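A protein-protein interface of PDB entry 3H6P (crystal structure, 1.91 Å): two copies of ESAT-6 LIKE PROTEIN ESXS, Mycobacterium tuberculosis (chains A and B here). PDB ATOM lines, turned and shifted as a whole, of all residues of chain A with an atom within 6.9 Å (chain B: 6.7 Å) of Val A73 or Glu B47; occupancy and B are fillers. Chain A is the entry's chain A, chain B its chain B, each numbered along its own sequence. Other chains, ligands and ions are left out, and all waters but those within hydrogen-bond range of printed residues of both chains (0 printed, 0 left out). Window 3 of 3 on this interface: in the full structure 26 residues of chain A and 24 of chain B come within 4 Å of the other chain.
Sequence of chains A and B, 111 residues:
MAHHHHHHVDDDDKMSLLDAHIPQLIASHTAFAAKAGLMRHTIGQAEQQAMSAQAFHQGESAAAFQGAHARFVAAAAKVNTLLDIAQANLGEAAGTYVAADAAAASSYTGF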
ATOM      1  N   PHE A  65      -0.994  33.880  -6.984  1.00  0.00           N
ATOM      2  CA  PHE A  65      -1.705  32.604  -7.016  1.00  0.00           C
ATOM      3  C   PHE A  65      -2.662  32.404  -5.824  1.00  0.00           C
ATOM      4  O   PHE A  65      -3.800  31.947  -5.991  1.00  0.00           O
ATOM      5  CB  PHE A  65      -0.739  31.421  -7.059  1.00  0.00           C
ATOM      6  CG  PHE A  65      -1.445  30.109  -7.066  1.00  0.00           C
ATOM      7  CD1 PHE A  65      -2.029  29.644  -8.227  1.00  0.00           C
ATOM      8  CD2 PHE A  65      -1.570  29.360  -5.900  1.00  0.00           C
ATOM      9  CE1 PHE A  65      -2.730  28.445  -8.225  1.00  0.00           C
ATOM     10  CE2 PHE A  65      -2.260  28.167  -5.897  1.00  0.00           C
ATOM     11  CZ  PHE A  65      -2.829  27.713  -7.073  1.00  0.00           C
ATOM     12  N   ALA A  68      -5.724  34.706  -6.397  1.00  0.00           N
ATOM     13  CA  ALA A  68      -6.510  34.116  -7.466  1.00  0.00           C
ATOM     14  C   ALA A  68      -7.287  32.902  -6.969  1.00  0.00           C
ATOM     15  O   ALA A  68      -8.481  32.759  -7.261  1.00  0.00           O
ATOM     16  CB  ALA A  68      -5.597  33.727  -8.633  1.00  0.00           C
ATOM     17  N   HIS A  69      -6.606  32.034  -6.223  1.00  0.00           N
ATOM     18  CA  HIS A  69      -7.196  30.797  -5.704  1.00  0.00           C
ATOM     19  C   HIS A  69      -8.347  31.075  -4.747  1.00  0.00           C
ATOM     20  O   HIS A  69      -9.401  30.432  -4.826  1.00  0.00           O
ATOM     21  CB  HIS A  69      -6.126  29.925  -5.034  1.00  0.00           C
ATOM     22  CG  HIS A  69      -6.594  28.543  -4.687  1.00  0.00           C
ATOM     23  ND1 HIS A  69      -5.901  27.717  -3.832  1.00  0.00           N
ATOM     24  CD2 HIS A  69      -7.670  27.834  -5.102  1.00  0.00           C
ATOM     25  CE1 HIS A  69      -6.544  26.568  -3.715  1.00  0.00           C
ATOM     26  NE2 HIS A  69      -7.622  26.615  -4.478  1.00  0.00           N
ATOM     27  N   ALA A  70      -8.150  32.033  -3.853  1.00  0.00           N
ATOM     28  CA  ALA A  70      -9.208  32.519  -2.984  1.00  0.00           C
ATOM     29  C   ALA A  70     -10.412  33.044  -3.793  1.00  0.00           C
ATOM     30  O   ALA A  70     -11.560  32.714  -3.477  1.00  0.00           O
ATOM     31  CB  ALA A  70      -8.642  33.606  -2.030  1.00  0.00           C
ATOM     32  N   ARG A  71     -10.153  33.818  -4.850  1.00  0.00           N
ATOM     33  CA  ARG A  71     -11.223  34.362  -5.688  1.00  0.00           C
ATOM     34  C   ARG A  71     -11.970  33.271  -6.439  1.00  0.00           C
ATOM     35  O   ARG A  71     -13.202  33.349  -6.619  1.00  0.00           O
ATOM     36  CB  ARG A  71     -10.703  35.414  -6.671  1.00  0.00           C
ATOM     37  CG  ARG A  71     -10.317  36.725  -5.995  1.00  0.00           C
ATOM     38  CD  ARG A  71     -10.077  37.830  -6.998  1.00  0.00           C
ATOM     39  NE  ARG A  71      -9.013  37.515  -7.951  1.00  0.00           N
ATOM     40  CZ  ARG A  71      -7.710  37.693  -7.726  1.00  0.00           C
ATOM     41  NH1 ARG A  71      -7.278  38.160  -6.560  1.00  0.00           N
ATOM     42  NH2 ARG A  71      -6.825  37.377  -8.669  1.00  0.00           N
ATOM     43  N   PHE A  72     -11.227  32.266  -6.881  1.00  0.00           N
ATOM     44  CA  PHE A  72     -11.803  31.102  -7.559  1.00  0.00           C
ATOM     45  C   PHE A  72     -12.767  30.318  -6.638  1.00  0.00           C
ATOM     46  O   PHE A  72     -13.879  29.958  -7.037  1.00  0.00           O
ATOM     47  CB  PHE A  72     -10.668  30.182  -8.057  1.00  0.00           C
ATOM     48  CG  PHE A  72     -11.158  28.941  -8.776  1.00  0.00           C
ATOM     49  CD1 PHE A  72     -11.265  28.915 -10.153  1.00  0.00           C
ATOM     50  CD2 PHE A  72     -11.508  27.808  -8.069  1.00  0.00           C
ATOM     51  CE1 PHE A  72     -11.721  27.751 -10.819  1.00  0.00           C
ATOM     52  CE2 PHE A  72     -11.969  26.664  -8.727  1.00  0.00           C
ATOM     53  CZ  PHE A  72     -12.053  26.639 -10.092  1.00  0.00           C
ATOM     54  N   VAL A  73     -12.315  30.046  -5.420  1.00  0.00           N
ATOM     55  CA  VAL A  73     -13.114  29.354  -4.410  1.00  0.00           C
ATOM     56  C   VAL A  73     -14.392  30.154  -4.085  1.00  0.00           C
ATOM     57  O   VAL A  73     -15.485  29.585  -4.050  1.00  0.00           O
ATOM     58  CB  VAL A  73     -12.252  29.059  -3.168  1.00  0.00           C
ATOM     59  CG1 VAL A  73     -13.086  28.613  -1.976  1.00  0.00           C
ATOM     60  CG2 VAL A  73     -11.210  28.006  -3.523  1.00  0.00           C
ATOM     61  N   ALA A  74     -14.265  31.462  -3.895  1.00  0.00           N
ATOM     62  CA  ALA A  74     -15.445  32.309  -3.622  1.00  0.00           C
ATOM     63  C   ALA A  74     -16.431  32.257  -4.784  1.00  0.00           C
ATOM     64  O   ALA A  74     -17.635  32.101  -4.575  1.00  0.00           O
ATOM     65  CB  ALA A  74     -15.031  33.740  -3.343  1.00  0.00           C
ATOM     66  N   ALA A  75     -15.922  32.342  -6.017  1.00  0.00           N
ATOM     67  CA  ALA A  75     -16.776  32.281  -7.225  1.00  0.00           C
ATOM     68  C   ALA A  75     -17.477  30.932  -7.376  1.00  0.00           C
ATOM     69  O   ALA A  75     -18.666  30.873  -7.722  1.00  0.00           O
ATOM     70  CB  ALA A  75     -15.952  32.591  -8.496  1.00  0.00           C
ATOM     71  N   ALA A  76     -16.745  29.854  -7.117  1.00  0.00           N
ATOM     72  CA  ALA A  76     -17.301  28.508  -7.162  1.00  0.00           C
ATOM     73  C   ALA A  76     -18.446  28.312  -6.158  1.00  0.00           C
ATOM     74  O   ALA A  76     -19.457  27.660  -6.476  1.00  0.00           O
ATOM     75  CB  ALA A  76     -16.206  27.478  -6.953  1.00  0.00           C
ATOM     76  N   ALA A  77     -18.288  28.847  -4.952  1.00  0.00           N
ATOM     77  CA  ALA A  77     -19.371  28.830  -3.961  1.00  0.00           C
ATOM     78  C   ALA A  77     -20.632  29.505  -4.533  1.00  0.00           C
ATOM     79  O   ALA A  77     -21.747  29.002  -4.375  1.00  0.00           O
ATOM     80  CB  ALA A  77     -18.917  29.540  -2.662  1.00  0.00           C
ATOM     81  N   LYS A  78     -20.453  30.615  -5.241  1.00  0.00           N
ATOM     82  CA  LYS A  78     -21.600  31.336  -5.803  1.00  0.00           C
ATOM     83  C   LYS A  78     -22.238  30.514  -6.906  1.00  0.00           C
ATOM     84  O   LYS A  78     -23.446  30.432  -6.998  1.00  0.00           O
ATOM     85  CB  LYS A  78     -21.182  32.701  -6.325  1.00  0.00           C
ATOM     86  CG  LYS A  78     -20.723  33.636  -5.236  1.00  0.00           C
ATOM     87  CD  LYS A  78     -20.369  35.008  -5.781  1.00  0.00           C
ATOM     88  CE  LYS A  78     -19.410  35.743  -4.856  1.00  0.00           C
ATOM     89  NZ  LYS A  78     -18.976  37.047  -5.444  1.00  0.00           N
ATOM     90  N   THR B  42     -16.146  19.887 -13.351  1.00  0.00           N
ATOM     91  CA  THR B  42     -15.180  20.673 -14.112  1.00  0.00           C
ATOM     92  C   THR B  42     -14.533  21.752 -13.250  1.00  0.00           C
ATOM     93  O   THR B  42     -13.353  22.022 -13.395  1.00  0.00           O
ATOM     94  CB  THR B  42     -15.850  21.243 -15.379  1.00  0.00           C
ATOM     95  OG1 THR B  42     -16.371  20.148 -16.130  1.00  0.00           O
ATOM     96  CG2 THR B  42     -14.880  22.040 -16.271  1.00  0.00           C
ATOM     97  N   ILE B  43     -15.282  22.331 -12.318  1.00  0.00           N
ATOM     98  CA  ILE B  43     -14.729  23.332 -11.404  1.00  0.00           C
ATOM     99  C   ILE B  43     -13.632  22.712 -10.515  1.00  0.00           C
ATOM    100  O   ILE B  43     -12.555  23.283 -10.358  1.00  0.00           O
ATOM    101  CB  ILE B  43     -15.817  23.981 -10.542  1.00  0.00           C
ATOM    102  CG1 ILE B  43     -16.724  24.875 -11.393  1.00  0.00           C
ATOM    103  CG2 ILE B  43     -15.192  24.796  -9.420  1.00  0.00           C
ATOM    104  CD1 ILE B  43     -17.985  25.387 -10.632  1.00  0.00           C
ATOM    105  N   GLY B  44     -13.890  21.523  -9.989  1.00  0.00           N
ATOM    106  CA  GLY B  44     -12.907  20.795  -9.190  1.00  0.00           C
ATOM    107  C   GLY B  44     -11.681  20.405  -9.988  1.00  0.00           C
ATOM    108  O   GLY B  44     -10.553  20.514  -9.495  1.00  0.00           O
ATOM    109  N   GLN B  45     -11.885  19.974 -11.223  1.00  0.00           N
ATOM    110  CA  GLN B  45     -10.782  19.604 -12.105  1.00  0.00           C
ATOM    111  C   GLN B  45      -9.916  20.795 -12.475  1.00  0.00           C
ATOM    112  O   GLN B  45      -8.685  20.705 -12.423  1.00  0.00           O
ATOM    113  CB  GLN B  45     -11.300  18.921 -13.372  1.00  0.00           C
ATOM    114  CG  GLN B  45     -11.777  17.519 -13.121  1.00  0.00           C
ATOM    115  CD  GLN B  45     -10.753  16.716 -12.327  1.00  0.00           C
ATOM    116  OE1 GLN B  45      -9.627  16.484 -12.797  1.00  0.00           O
ATOM    117  NE2 GLN B  45     -11.118  16.333 -11.096  1.00  0.00           N
ATOM    118  N   ALA B  46     -10.561  21.897 -12.846  1.00  0.00           N
ATOM    119  CA  ALA B  46      -9.872  23.146 -13.137  1.00  0.00           C
ATOM    120  C   ALA B  46      -9.013  23.626 -11.959  1.00  0.00           C
ATOM    121  O   ALA B  46      -7.874  24.054 -12.157  1.00  0.00           O
ATOM    122  CB  ALA B  46     -10.875  24.219 -13.544  1.00  0.00           C
ATOM    123  N   GLU B  47      -9.563  23.558 -10.747  1.00  0.00           N
ATOM    124  CA  GLU B  47      -8.821  23.919  -9.555  1.00  0.00           C
ATOM    125  C   GLU B  47      -7.560  23.068  -9.390  1.00  0.00           C
ATOM    126  O   GLU B  47      -6.479  23.612  -9.162  1.00  0.00           O
ATOM    127  CB  GLU B  47      -9.706  23.801  -8.302  1.00  0.00           C
ATOM    128  CG  GLU B  47      -9.052  24.376  -7.050  1.00  0.00           C
ATOM    129  CD  GLU B  47      -9.835  24.144  -5.782  1.00  0.00           C
ATOM    130  OE1 GLU B  47     -10.685  23.221  -5.738  1.00  0.00           O
ATOM    131  OE2 GLU B  47      -9.589  24.885  -4.809  1.00  0.00           O
ATOM    132  N   GLN B  48      -7.708  21.746  -9.461  1.00  0.00           N
ATOM    133  CA  GLN B  48      -6.561  20.843  -9.280  1.00  0.00           C
ATOM    134  C   GLN B  48      -5.500  21.059 -10.355  1.00  0.00           C
ATOM    135  O   GLN B  48      -4.310  21.101 -10.061  1.00  0.00           O
ATOM    136  CB  GLN B  48      -7.011  19.387  -9.308  1.00  0.00           C
ATOM    137  CG  GLN B  48      -7.844  18.976  -8.122  1.00  0.00           C
ATOM    138  CD  GLN B  48      -7.139  19.175  -6.785  1.00  0.00           C
ATOM    139  OE1 GLN B  48      -5.922  18.971  -6.665  1.00  0.00           O
ATOM    140  NE2 GLN B  48      -7.907  19.579  -5.767  1.00  0.00           N
ATOM    141  N   GLN B  49      -5.946  21.194 -11.590  1.00  0.00           N
ATOM    142  CA  GLN B  49      -5.060  21.492 -12.734  1.00  0.00           C
ATOM    143  C   GLN B  49      -4.258  22.785 -12.549  1.00  0.00           C
ATOM    144  O   GLN B  49      -3.058  22.843 -12.872  1.00  0.00           O
ATOM    145  CB  GLN B  49      -5.892  21.603 -14.007  1.00  0.00           C
ATOM    146  CG  GLN B  49      -5.110  21.780 -15.309  1.00  0.00           C
ATOM    147  CD  GLN B  49      -4.735  23.203 -15.619  1.00  0.00           C
ATOM    148  OE1 GLN B  49      -3.634  23.475 -16.108  1.00  0.00           O
ATOM    149  NE2 GLN B  49      -5.635  24.126 -15.338  1.00  0.00           N
ATOM    150  N   ALA B  50      -4.943  23.827 -12.080  1.00  0.00           N
ATOM    151  CA  ALA B  50      -4.325  25.151 -11.892  1.00  0.00           C
ATOM    152  C   ALA B  50      -3.307  25.139 -10.741  1.00  0.00           C
ATOM    153  O   ALA B  50      -2.282  25.804 -10.820  1.00  0.00           O
ATOM    154  CB  ALA B  50      -5.403  26.201 -11.646  1.00  0.00           C
ATOM    155  N   MET B  51      -3.616  24.406  -9.672  1.00  0.00           N
ATOM    156  CA  MET B  51      -2.721  24.258  -8.538  1.00  0.00           C
ATOM    157  C   MET B  51      -1.445  23.528  -8.957  1.00  0.00           C
ATOM    158  O   MET B  51      -0.334  23.923  -8.572  1.00  0.00           O
ATOM    159  CB  MET B  51      -3.402  23.487  -7.386  1.00  0.00           C
ATOM    160  CG  MET B  51      -4.590  24.216  -6.729  1.00  0.00           C
ATOM    161  SD  MET B  51      -5.545  23.197  -5.556  1.00  0.00           S
ATOM    162  CE  MET B  51      -4.394  23.155  -4.208  1.00  0.00           C
ATOM    163  N   SER B  52      -1.623  22.464  -9.742  1.00  0.00           N
ATOM    164  CA  SER B  52      -0.519  21.708 -10.315  1.00  0.00           C
ATOM    165  C   SER B  52       0.307  22.565 -11.291  1.00  0.00           C
ATOM    166  O   SER B  52       1.534  22.521 -11.268  1.00  0.00           O
ATOM    167  CB  SER B  52      -1.059  20.450 -10.998  1.00  0.00           C
ATOM    168  OG  SER B  52      -0.032  19.786 -11.708  1.00  0.00           O
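The side-chain carboxylate (OE2) of Glu B47 lies within hydrogen-bond range of a ring nitrogen (NE2) of His A69, at 2.6 Å.
Among the printed residues, pairs that only touch across the chains: Phe A65 with Ala B50 (3.7 Å), Phe A65 with Met B51 (3.8 Å), His A69 with Met B51 (3.97 Å), Phe A72 with Ile B43 (3.4 Å), Phe A72 with Glu B47 (3.7 Å), Val A73 with Glu B47 (3.7 Å) and Ala A76 with Ile B43 (3.8 Å).
Of chain B, only Glu B47 (3.7 Å) comes within 4 Å of Val A73. Glu B47 touches just these residues of chain A: His A69 (2.6 Å), Phe A72 (3.7 Å) and Val A73 (3.7 Å). Of the printed residues of chain A, Ile B43 touches Phe A72 and Ala A76. Of the printed residues of chain B, Phe A72 touches Ile B43 and Glu B47. Thr B42 touches none of the printed residues of chain A. The nearest residue of chain A that does not touch Glu B47 is Phe A65 (5.9 Å).
Along chain A the printed residues that touch a printed residue of chain B span positions 65 to 76. Of the 11 printed residues of chain B, 4 touch a printed residue of chain A. Among the printed residues, no Asp or Glu carboxylate lies within 4 Å of a Lys or Arg side-chain nitrogen of the other chain.
No position is printed for both chains.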
